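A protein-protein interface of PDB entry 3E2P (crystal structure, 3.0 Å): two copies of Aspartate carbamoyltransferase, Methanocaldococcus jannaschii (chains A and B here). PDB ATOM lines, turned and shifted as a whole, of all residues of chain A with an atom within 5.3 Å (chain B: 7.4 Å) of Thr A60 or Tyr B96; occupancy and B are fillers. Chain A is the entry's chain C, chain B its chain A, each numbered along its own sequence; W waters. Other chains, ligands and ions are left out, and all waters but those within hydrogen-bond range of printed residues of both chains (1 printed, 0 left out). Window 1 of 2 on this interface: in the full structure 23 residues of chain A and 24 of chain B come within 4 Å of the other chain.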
ATOM      1  N   ARG A  53     -15.629 -15.617  -9.299  1.00  0.00           N
ATOM      2  CA  ARG A  53     -14.993 -14.823 -10.352  1.00  0.00           C
ATOM      3  C   ARG A  53     -13.469 -14.830 -10.288  1.00  0.00           C
ATOM      4  O   ARG A  53     -12.804 -15.193 -11.254  1.00  0.00           O
ATOM      5  CB  ARG A  53     -15.486 -13.378 -10.313  1.00  0.00           C
ATOM      6  CG  ARG A  53     -16.954 -13.271 -10.578  1.00  0.00           C
ATOM      7  CD  ARG A  53     -17.420 -11.852 -10.835  1.00  0.00           C
ATOM      8  NE  ARG A  53     -18.875 -11.848 -10.847  1.00  0.00           N
ATOM      9  CZ  ARG A  53     -19.614 -12.219  -9.806  1.00  0.00           C
ATOM     10  NH1 ARG A  53     -19.025 -12.610  -8.673  1.00  0.00           N
ATOM     11  NH2 ARG A  53     -20.937 -12.232  -9.906  1.00  0.00           N
ATOM     12  N   ARG A  55     -11.504 -16.791  -8.597  1.00  0.00           N
ATOM     13  CA  ARG A  55     -10.983 -18.145  -8.727  1.00  0.00           C
ATOM     14  C   ARG A  55     -10.903 -18.553 -10.193  1.00  0.00           C
ATOM     15  O   ARG A  55      -9.847 -18.961 -10.663  1.00  0.00           O
ATOM     16  CB  ARG A  55     -11.854 -19.139  -7.976  1.00  0.00           C
ATOM     17  CG  ARG A  55     -11.411 -20.561  -8.153  1.00  0.00           C
ATOM     18  CD  ARG A  55     -12.304 -21.483  -7.373  1.00  0.00           C
ATOM     19  NE  ARG A  55     -13.681 -21.489  -7.853  1.00  0.00           N
ATOM     20  CZ  ARG A  55     -14.049 -21.982  -9.037  1.00  0.00           C
ATOM     21  NH1 ARG A  55     -13.125 -22.507  -9.849  1.00  0.00           N
ATOM     22  NH2 ARG A  55     -15.332 -21.945  -9.416  1.00  0.00           N
ATOM     23  N   LEU A  56     -12.014 -18.441 -10.913  1.00  0.00           N
ATOM     24  CA  LEU A  56     -12.033 -18.803 -12.316  1.00  0.00           C
ATOM     25  C   LEU A  56     -10.991 -18.066 -13.138  1.00  0.00           C
ATOM     26  O   LEU A  56     -10.371 -18.648 -14.038  1.00  0.00           O
ATOM     27  CB  LEU A  56     -13.413 -18.547 -12.925  1.00  0.00           C
ATOM     28  CG  LEU A  56     -14.494 -19.576 -12.617  1.00  0.00           C
ATOM     29  CD1 LEU A  56     -15.695 -19.257 -13.442  1.00  0.00           C
ATOM     30  CD2 LEU A  56     -14.012 -20.983 -12.943  1.00  0.00           C
ATOM     31  N   SER A  57     -10.805 -16.784 -12.846  1.00  0.00           N
ATOM     32  CA  SER A  57      -9.835 -15.975 -13.577  1.00  0.00           C
ATOM     33  C   SER A  57      -8.441 -16.588 -13.432  1.00  0.00           C
ATOM     34  O   SER A  57      -7.788 -16.931 -14.423  1.00  0.00           O
ATOM     35  CB  SER A  57      -9.841 -14.546 -13.038  1.00  0.00           C
ATOM     36  OG  SER A  57      -9.086 -13.683 -13.866  1.00  0.00           O
ATOM     37  N   PHE A  58      -7.997 -16.729 -12.191  1.00  0.00           N
ATOM     38  CA  PHE A  58      -6.697 -17.308 -11.902  1.00  0.00           C
ATOM     39  C   PHE A  58      -6.587 -18.749 -12.353  1.00  0.00           C
ATOM     40  O   PHE A  58      -5.525 -19.190 -12.760  1.00  0.00           O
ATOM     41  CB  PHE A  58      -6.419 -17.247 -10.410  1.00  0.00           C
ATOM     42  CG  PHE A  58      -5.772 -15.977  -9.970  1.00  0.00           C
ATOM     43  CD1 PHE A  58      -4.422 -15.758 -10.210  1.00  0.00           C
ATOM     44  CD2 PHE A  58      -6.510 -14.997  -9.323  1.00  0.00           C
ATOM     45  CE1 PHE A  58      -3.814 -14.578  -9.809  1.00  0.00           C
ATOM     46  CE2 PHE A  58      -5.916 -13.815  -8.920  1.00  0.00           C
ATOM     47  CZ  PHE A  58      -4.562 -13.603  -9.163  1.00  0.00           C
ATOM     48  N   GLU A  59      -7.681 -19.492 -12.268  1.00  0.00           N
ATOM     49  CA  GLU A  59      -7.679 -20.887 -12.672  1.00  0.00           C
ATOM     50  C   GLU A  59      -7.437 -20.960 -14.170  1.00  0.00           C
ATOM     51  O   GLU A  59      -6.616 -21.747 -14.639  1.00  0.00           O
ATOM     52  CB  GLU A  59      -9.014 -21.531 -12.318  1.00  0.00           C
ATOM     53  CG  GLU A  59      -9.036 -23.023 -12.447  1.00  0.00           C
ATOM     54  CD  GLU A  59     -10.285 -23.603 -11.849  1.00  0.00           C
ATOM     55  OE1 GLU A  59     -10.551 -23.329 -10.654  1.00  0.00           O
ATOM     56  OE2 GLU A  59     -10.999 -24.327 -12.572  1.00  0.00           O
ATOM     57  N   THR A  60      -8.147 -20.121 -14.913  1.00  0.00           N
ATOM     58  CA  THR A  60      -8.009 -20.096 -16.361  1.00  0.00           C
ATOM     59  C   THR A  60      -6.580 -19.746 -16.724  1.00  0.00           C
ATOM     60  O   THR A  60      -5.936 -20.451 -17.496  1.00  0.00           O
ATOM     61  CB  THR A  60      -8.972 -19.073 -17.003  1.00  0.00           C
ATOM     62  OG1 THR A  60     -10.323 -19.455 -16.733  1.00  0.00           O
ATOM     63  CG2 THR A  60      -8.784 -19.032 -18.500  1.00  0.00           C
ATOM     64  N   ALA A  61      -6.089 -18.657 -16.151  1.00  0.00           N
ATOM     65  CA  ALA A  61      -4.734 -18.202 -16.406  1.00  0.00           C
ATOM     66  C   ALA A  61      -3.702 -19.307 -16.184  1.00  0.00           C
ATOM     67  O   ALA A  61      -2.856 -19.550 -17.041  1.00  0.00           O
ATOM     68  CB  ALA A  61      -4.417 -17.009 -15.516  1.00  0.00           C
ATOM     69  N   MET A  62      -3.776 -19.976 -15.038  1.00  0.00           N
ATOM     70  CA  MET A  62      -2.836 -21.039 -14.713  1.00  0.00           C
ATOM     71  C   MET A  62      -2.897 -22.174 -15.731  1.00  0.00           C
ATOM     72  O   MET A  62      -1.865 -22.690 -16.176  1.00  0.00           O
ATOM     73  CB  MET A  62      -3.118 -21.582 -13.318  1.00  0.00           C
ATOM     74  CG  MET A  62      -2.147 -22.643 -12.864  1.00  0.00           C
ATOM     75  SD  MET A  62      -0.461 -22.049 -12.771  1.00  0.00           S
ATOM     76  CE  MET A  62       0.418 -23.564 -12.396  1.00  0.00           C
ATOM     77  N   LYS A  63      -4.108 -22.558 -16.114  1.00  0.00           N
ATOM     78  CA  LYS A  63      -4.275 -23.633 -17.078  1.00  0.00           C
ATOM     79  C   LYS A  63      -3.835 -23.238 -18.475  1.00  0.00           C
ATOM     80  O   LYS A  63      -3.377 -24.083 -19.239  1.00  0.00           O
ATOM     81  CB  LYS A  63      -5.722 -24.125 -17.065  1.00  0.00           C
ATOM     82  CG  LYS A  63      -6.042 -24.828 -15.754  1.00  0.00           C
ATOM     83  CD  LYS A  63      -7.476 -25.261 -15.635  1.00  0.00           C
ATOM     84  CE  LYS A  63      -7.681 -25.994 -14.320  1.00  0.00           C
ATOM     85  NZ  LYS A  63      -9.077 -26.414 -14.100  1.00  0.00           N
ATOM     86  N   ARG A  64      -3.958 -21.958 -18.810  1.00  0.00           N
ATOM     87  CA  ARG A  64      -3.526 -21.478 -20.119  1.00  0.00           C
ATOM     88  C   ARG A  64      -2.012 -21.592 -20.251  1.00  0.00           C
ATOM     89  O   ARG A  64      -1.489 -21.748 -21.354  1.00  0.00           O
ATOM     90  CB  ARG A  64      -3.931 -20.028 -20.330  1.00  0.00           C
ATOM     91  CG  ARG A  64      -5.380 -19.837 -20.682  1.00  0.00           C
ATOM     92  CD  ARG A  64      -5.734 -20.530 -21.969  1.00  0.00           C
ATOM     93  NE  ARG A  64      -7.114 -20.271 -22.365  1.00  0.00           N
ATOM     94  CZ  ARG A  64      -7.759 -20.992 -23.276  1.00  0.00           C
ATOM     95  NH1 ARG A  64      -7.146 -22.010 -23.881  1.00  0.00           N
ATOM     96  NH2 ARG A  64      -9.023 -20.717 -23.585  1.00  0.00           N
ATOM     97  N   LEU A  65      -1.310 -21.509 -19.126  1.00  0.00           N
ATOM     98  CA  LEU A  65       0.137 -21.632 -19.138  1.00  0.00           C
ATOM     99  C   LEU A  65       0.523 -23.087 -19.010  1.00  0.00           C
ATOM    100  O   LEU A  65       1.696 -23.402 -18.825  1.00  0.00           O
ATOM    101  CB  LEU A  65       0.763 -20.845 -17.993  1.00  0.00           C
ATOM    102  CG  LEU A  65       0.693 -19.329 -18.121  1.00  0.00           C
ATOM    103  CD1 LEU A  65       1.250 -18.699 -16.874  1.00  0.00           C
ATOM    104  CD2 LEU A  65       1.464 -18.882 -19.342  1.00  0.00           C
ATOM    105  N   SER A 285     -12.327  -7.465 -18.714  1.00  0.00           N
ATOM    106  CA  SER A 285     -12.534  -8.759 -18.055  1.00  0.00           C
ATOM    107  C   SER A 285     -11.534  -9.781 -18.571  1.00  0.00           C
ATOM    108  O   SER A 285     -10.899 -10.500 -17.804  1.00  0.00           O
ATOM    109  CB  SER A 285     -13.951  -9.272 -18.314  1.00  0.00           C
ATOM    110  OG  SER A 285     -14.073 -10.612 -17.879  1.00  0.00           O
ATOM    111  N   PHE A 286     -11.418  -9.827 -19.891  1.00  0.00           N
ATOM    112  CA  PHE A 286     -10.518 -10.723 -20.584  1.00  0.00           C
ATOM    113  C   PHE A 286      -9.076 -10.455 -20.212  1.00  0.00           C
ATOM    114  O   PHE A 286      -8.321 -11.388 -19.946  1.00  0.00           O
ATOM    115  CB  PHE A 286     -10.677 -10.558 -22.084  1.00  0.00           C
ATOM    116  CG  PHE A 286      -9.596 -11.208 -22.854  1.00  0.00           C
ATOM    117  CD1 PHE A 286      -9.525 -12.591 -22.937  1.00  0.00           C
ATOM    118  CD2 PHE A 286      -8.600 -10.446 -23.448  1.00  0.00           C
ATOM    119  CE1 PHE A 286      -8.477 -13.212 -23.598  1.00  0.00           C
ATOM    120  CE2 PHE A 286      -7.546 -11.055 -24.109  1.00  0.00           C
ATOM    121  CZ  PHE A 286      -7.485 -12.442 -24.184  1.00  0.00           C
ATOM    122  N   ILE A 289      -6.963 -12.378 -17.675  1.00  0.00           N
ATOM    123  CA  ILE A 289      -6.306 -13.642 -17.964  1.00  0.00           C
ATOM    124  C   ILE A 289      -4.823 -13.470 -18.303  1.00  0.00           C
ATOM    125  O   ILE A 289      -3.959 -14.105 -17.697  1.00  0.00           O
ATOM    126  CB  ILE A 289      -7.013 -14.390 -19.129  1.00  0.00           C
ATOM    127  CG1 ILE A 289      -8.478 -14.665 -18.763  1.00  0.00           C
ATOM    128  CG2 ILE A 289      -6.281 -15.707 -19.429  1.00  0.00           C
ATOM    129  CD1 ILE A 289      -8.686 -15.541 -17.529  1.00  0.00           C
ATOM    130  N   ILE B  42     -10.184 -25.335 -23.238  1.00  0.00           N
ATOM    131  CA  ILE B  42     -10.773 -25.248 -21.916  1.00  0.00           C
ATOM    132  C   ILE B  42     -12.296 -25.263 -22.010  1.00  0.00           C
ATOM    133  O   ILE B  42     -12.910 -24.479 -22.736  1.00  0.00           O
ATOM    134  CB  ILE B  42     -10.365 -23.945 -21.191  1.00  0.00           C
ATOM    135  CG1 ILE B  42      -8.855 -23.936 -20.913  1.00  0.00           C
ATOM    136  CG2 ILE B  42     -11.181 -23.790 -19.900  1.00  0.00           C
ATOM    137  CD1 ILE B  42      -8.378 -22.690 -20.154  1.00  0.00           C
ATOM    138  N   ALA B  44     -15.911 -24.816 -20.109  1.00  0.00           N
ATOM    139  CA  ALA B  44     -16.487 -24.154 -18.946  1.00  0.00           C
ATOM    140  C   ALA B  44     -17.829 -24.785 -18.605  1.00  0.00           C
ATOM    141  O   ALA B  44     -18.725 -24.872 -19.448  1.00  0.00           O
ATOM    142  CB  ALA B  44     -16.670 -22.683 -19.215  1.00  0.00           C
ATOM    143  N   ILE B  70     -12.867 -25.668 -16.395  1.00  0.00           N
ATOM    144  CA  ILE B  70     -13.067 -24.731 -15.290  1.00  0.00           C
ATOM    145  C   ILE B  70     -14.554 -24.861 -14.963  1.00  0.00           C
ATOM    146  O   ILE B  70     -15.406 -24.872 -15.865  1.00  0.00           O
ATOM    147  CB  ILE B  70     -12.741 -23.252 -15.653  1.00  0.00           C
ATOM    148  CG1 ILE B  70     -13.626 -22.759 -16.801  1.00  0.00           C
ATOM    149  CG2 ILE B  70     -11.269 -23.121 -15.996  1.00  0.00           C
ATOM    150  CD1 ILE B  70     -13.391 -21.312 -17.166  1.00  0.00           C
ATOM    151  N   MET B  72     -18.058 -23.744 -12.648  1.00  0.00           N
ATOM    152  CA  MET B  72     -18.774 -22.676 -11.975  1.00  0.00           C
ATOM    153  C   MET B  72     -20.212 -23.157 -11.805  1.00  0.00           C
ATOM    154  O   MET B  72     -21.028 -23.031 -12.717  1.00  0.00           O
ATOM    155  CB  MET B  72     -18.746 -21.433 -12.846  1.00  0.00           C
ATOM    156  CG  MET B  72     -19.685 -20.355 -12.411  1.00  0.00           C
ATOM    157  SD  MET B  72     -19.741 -19.064 -13.660  1.00  0.00           S
ATOM    158  CE  MET B  72     -18.736 -17.803 -12.860  1.00  0.00           C
ATOM    159  N   ILE B  90     -22.212 -15.226 -19.251  1.00  0.00           N
ATOM    160  CA  ILE B  90     -21.860 -15.923 -20.491  1.00  0.00           C
ATOM    161  C   ILE B  90     -20.787 -15.156 -21.250  1.00  0.00           C
ATOM    162  O   ILE B  90     -19.870 -15.766 -21.796  1.00  0.00           O
ATOM    163  CB  ILE B  90     -23.074 -16.115 -21.425  1.00  0.00           C
ATOM    164  CG1 ILE B  90     -23.975 -17.227 -20.884  1.00  0.00           C
ATOM    165  CG2 ILE B  90     -22.607 -16.445 -22.842  1.00  0.00           C
ATOM    166  CD1 ILE B  90     -23.288 -18.559 -20.754  1.00  0.00           C
ATOM    167  N   ARG B  91     -20.889 -13.824 -21.279  1.00  0.00           N
ATOM    168  CA  ARG B  91     -19.886 -13.013 -21.956  1.00  0.00           C
ATOM    169  C   ARG B  91     -18.517 -13.095 -21.286  1.00  0.00           C
ATOM    170  O   ARG B  91     -17.504 -13.193 -21.962  1.00  0.00           O
ATOM    171  CB  ARG B  91     -20.354 -11.565 -22.070  1.00  0.00           C
ATOM    172  CG  ARG B  91     -21.279 -11.396 -23.254  1.00  0.00           C
ATOM    173  CD  ARG B  91     -21.690  -9.966 -23.487  1.00  0.00           C
ATOM    174  NE  ARG B  91     -22.608  -9.506 -22.458  1.00  0.00           N
ATOM    175  CZ  ARG B  91     -23.402  -8.448 -22.581  1.00  0.00           C
ATOM    176  NH1 ARG B  91     -23.390  -7.739 -23.700  1.00  0.00           N
ATOM    177  NH2 ARG B  91     -24.202  -8.094 -21.581  1.00  0.00           N
ATOM    178  N   VAL B  92     -18.478 -13.079 -19.962  1.00  0.00           N
ATOM    179  CA  VAL B  92     -17.200 -13.173 -19.276  1.00  0.00           C
ATOM    180  C   VAL B  92     -16.568 -14.540 -19.453  1.00  0.00           C
ATOM    181  O   VAL B  92     -15.404 -14.632 -19.814  1.00  0.00           O
ATOM    182  CB  VAL B  92     -17.337 -12.893 -17.781  1.00  0.00           C
ATOM    183  CG1 VAL B  92     -15.996 -13.111 -17.092  1.00  0.00           C
ATOM    184  CG2 VAL B  92     -17.808 -11.468 -17.573  1.00  0.00           C
ATOM    185  N   ILE B  93     -17.329 -15.597 -19.188  1.00  0.00           N
ATOM    186  CA  ILE B  93     -16.827 -16.957 -19.329  1.00  0.00           C
ATOM    187  C   ILE B  93     -16.477 -17.216 -20.791  1.00  0.00           C
ATOM    188  O   ILE B  93     -15.494 -17.882 -21.091  1.00  0.00           O
ATOM    189  CB  ILE B  93     -17.887 -17.992 -18.900  1.00  0.00           C
ATOM    190  CG1 ILE B  93     -18.248 -17.813 -17.422  1.00  0.00           C
ATOM    191  CG2 ILE B  93     -17.378 -19.404 -19.182  1.00  0.00           C
ATOM    192  CD1 ILE B  93     -17.138 -18.087 -16.504  1.00  0.00           C
ATOM    193  N   SER B  94     -17.294 -16.690 -21.699  1.00  0.00           N
ATOM    194  CA  SER B  94     -17.080 -16.861 -23.134  1.00  0.00           C
ATOM    195  C   SER B  94     -15.672 -16.383 -23.493  1.00  0.00           C
ATOM    196  O   SER B  94     -15.013 -16.917 -24.384  1.00  0.00           O
ATOM    197  CB  SER B  94     -18.120 -16.041 -23.907  1.00  0.00           C
ATOM    198  OG  SER B  94     -18.188 -16.409 -25.271  1.00  0.00           O
ATOM    199  N   GLY B  95     -15.219 -15.370 -22.777  1.00  0.00           N
ATOM    200  CA  GLY B  95     -13.911 -14.815 -23.028  1.00  0.00           C
ATOM    201  C   GLY B  95     -12.806 -15.630 -22.400  1.00  0.00           C
ATOM    202  O   GLY B  95     -11.661 -15.559 -22.843  1.00  0.00           O
ATOM    203  N   TYR B  96     -13.137 -16.407 -21.375  1.00  0.00           N
ATOM    204  CA  TYR B  96     -12.152 -17.243 -20.687  1.00  0.00           C
ATOM    205  C   TYR B  96     -11.921 -18.576 -21.386  1.00  0.00           C
ATOM    206  O   TYR B  96     -10.790 -18.924 -21.727  1.00  0.00           O
ATOM    207  CB  TYR B  96     -12.600 -17.561 -19.257  1.00  0.00           C
ATOM    208  CG  TYR B  96     -12.565 -16.414 -18.280  1.00  0.00           C
ATOM    209  CD1 TYR B  96     -12.288 -15.103 -18.696  1.00  0.00           C
ATOM    210  CD2 TYR B  96     -12.822 -16.633 -16.927  1.00  0.00           C
ATOM    211  CE1 TYR B  96     -12.271 -14.039 -17.776  1.00  0.00           C
ATOM    212  CE2 TYR B  96     -12.806 -15.583 -16.006  1.00  0.00           C
ATOM    213  CZ  TYR B  96     -12.528 -14.293 -16.439  1.00  0.00           C
ATOM    214  OH  TYR B  96     -12.484 -13.263 -15.535  1.00  0.00           O
ATOM    215  N   ALA B  97     -13.004 -19.323 -21.585  1.00  0.00           N
ATOM    216  CA  ALA B  97     -12.926 -20.648 -22.172  1.00  0.00           C
ATOM    217  C   ALA B  97     -13.107 -20.708 -23.655  1.00  0.00           C
ATOM    218  O   ALA B  97     -13.267 -19.683 -24.317  1.00  0.00           O
ATOM    219  CB  ALA B  97     -13.923 -21.564 -21.512  1.00  0.00           C
ATOM    220  N   ASP B  98     -13.099 -21.938 -24.165  1.00  0.00           N
ATOM    221  CA  ASP B  98     -13.216 -22.199 -25.588  1.00  0.00           C
ATOM    222  C   ASP B  98     -14.551 -22.811 -25.912  1.00  0.00           C
ATOM    223  O   ASP B  98     -14.993 -22.780 -27.059  1.00  0.00           O
ATOM    224  CB  ASP B  98     -12.076 -23.124 -26.035  1.00  0.00           C
ATOM    225  CG  ASP B  98     -10.695 -22.579 -25.650  1.00  0.00           C
ATOM    226  OD1 ASP B  98     -10.342 -21.473 -26.110  1.00  0.00           O
ATOM    227  OD2 ASP B  98      -9.967 -23.248 -24.882  1.00  0.00           O
ATOM    228  N   ILE B  99     -15.192 -23.370 -24.896  1.00  0.00           N
ATOM    229  CA  ILE B  99     -16.506 -23.976 -25.081  1.00  0.00           C
ATOM    230  C   ILE B  99     -17.252 -24.037 -23.733  1.00  0.00           C
ATOM    231  O   ILE B  99     -16.646 -24.239 -22.677  1.00  0.00           O
ATOM    232  CB  ILE B  99     -16.376 -25.380 -25.756  1.00  0.00           C
ATOM    233  CG1 ILE B  99     -17.757 -25.885 -26.175  1.00  0.00           C
ATOM    234  CG2 ILE B  99     -15.678 -26.347 -24.829  1.00  0.00           C
ATOM    235  CD1 ILE B  99     -17.736 -27.189 -26.942  1.00  0.00           C
ATOM    236  N   ILE B 100     -18.569 -23.849 -23.782  1.00  0.00           N
ATOM    237  CA  ILE B 100     -19.393 -23.826 -22.574  1.00  0.00           C
ATOM    238  C   ILE B 100     -20.572 -24.797 -22.537  1.00  0.00           C
ATOM    239  O   ILE B 100     -21.331 -24.918 -23.499  1.00  0.00           O
ATOM    240  CB  ILE B 100     -19.994 -22.411 -22.346  1.00  0.00           C
ATOM    241  CG1 ILE B 100     -18.876 -21.374 -22.187  1.00  0.00           C
ATOM    242  CG2 ILE B 100     -20.901 -22.420 -21.127  1.00  0.00           C
ATOM    243  CD1 ILE B 100     -19.372 -19.927 -22.130  1.00  0.00           C
ATOM    244  N   GLN B 118     -19.332 -15.973 -27.502  1.00  0.00           N
ATOM    245  CA  GLN B 118     -18.403 -15.916 -28.624  1.00  0.00           C
ATOM    246  C   GLN B 118     -17.796 -17.303 -28.661  1.00  0.00           C
ATOM    247  O   GLN B 118     -16.710 -17.503 -29.189  1.00  0.00           O
ATOM    248  CB  GLN B 118     -17.290 -14.890 -28.364  1.00  0.00           C
ATOM    249  CG  GLN B 118     -16.449 -15.215 -27.123  1.00  0.00           C
ATOM    250  CD  GLN B 118     -15.207 -14.348 -26.955  1.00  0.00           C
ATOM    251  OE1 GLN B 118     -15.290 -13.130 -26.829  1.00  0.00           O
ATOM    252  NE2 GLN B 118     -14.046 -14.985 -26.941  1.00  0.00           N
ATOM    253  N   VAL B 119     -18.511 -18.259 -28.085  1.00  0.00           N
ATOM    254  CA  VAL B 119     -18.037 -19.627 -27.999  1.00  0.00           C
ATOM    255  C   VAL B 119     -19.210 -20.604 -28.092  1.00  0.00           C
ATOM    256  O   VAL B 119     -20.341 -20.256 -27.758  1.00  0.00           O
ATOM    257  CB  VAL B 119     -17.300 -19.802 -26.675  1.00  0.00           C
ATOM    258  CG1 VAL B 119     -17.363 -21.220 -26.237  1.00  0.00           C
ATOM    259  CG2 VAL B 119     -15.855 -19.356 -26.820  1.00  0.00           C
HETATM  260  O   HOH W   1      -7.831 -17.522 -22.517  1.00  0.00           O
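CB of Ile B70 touches CD2 of Leu A56 (3.8 Å).
Met B72 touches Leu A56.
Leu A56 touches Ile B93 (CD1 to CD1, 3.6 Å).
OG of Ser A57 touches OH of Tyr B96, 3.8 Å away.
CA of Ile B70 touches OE2 of Glu A59, 3.4 Å away.
Thr A60 touches Ile B70 (OG1 to CD1, 3.6 Å).
CD2 of Tyr B96 touches OG1 of Thr A60, 3.8 Å away.
Val B92 touches Ser A285.
CE1 of Tyr B96 touches O of Ser A285 (3.8 Å).
Phe A286 touches Gly B95 (CD1 to O, 3.7 Å).
The side-chain carboxylate (OE2) of Glu A59 is in salt-bridge range of the side-chain amino group (NZ) of Lys A63 (3.2 Å).
The backbone NH (N) of Ile B99 sits at hydrogen-bond distance from the backbone carbonyl oxygen (O) of Ile B42 (3.3 Å).
O of Leu A56 sits at hydrogen-bond distance from OG1 of Thr A60, at 2.8 Å.
The backbone NH (N) of Ile B42 lies within hydrogen-bond range of the side-chain carboxylate (OD2) of Asp B98 (2.7 Å).
The side-chain carboxylate (OE1) of Glu A59 is in salt-bridge range of the guanidinium group (NH1) of Arg A55 (2.8 Å).
Of the printed residues of chain B, Thr A60 touches Ile B70 and Tyr B96.
Printed residues of chain B within 4 Å of Ile A289: Tyr B96 (3.8 Å).
Of the printed residues of chain A, Ile B42 touches Arg A64 (3.5 Å).
Of the printed residues of chain A, Val B92 touches Ser A285.
Of the printed residues of chain A, Ile B93 touches Leu A56.
The nearest residue of chain B that does not touch Thr A60 is Ile B42 (4.04 Å).
The nearest residue of chain A that does not touch Tyr B96 is Leu A56 (4.2 Å).
No position is printed for both chains.
Of the 14 pairs that touch across the chains among the printed residues, none has its exchanged pair printed and touching as well.
Water W1 lies within hydrogen-bond range of NE of Arg A64 and O of Tyr B96.
Hydrophobic or aromatic side chains of chain A within 4 Å of the printed part of chain B: Leu A56, Phe A286 and Ile A289.
Hydrophobic or aromatic side chains of chain B within 4 Å of the printed part of chain A: Ile B42, Ile B70, Met B72, Val B92, Ile B93 and Tyr B96.
Along chain B the printed residues that touch a printed residue of chain A span positions 42 to 98.
Among the printed residues, Asp or Glu carboxylates within 4 Å of a Lys or Arg side-chain nitrogen of the other chain: Arg A64 with Asp B98 (2.9 Å).
OD1 of Asp B98 lies within salt-bridge range of NH2 of Arg A64, 2.9 Å away.
The backbone carbonyl oxygen (O) of Tyr B96 sits at hydrogen-bond distance from the guanidinium group (NH2) of Arg A64.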
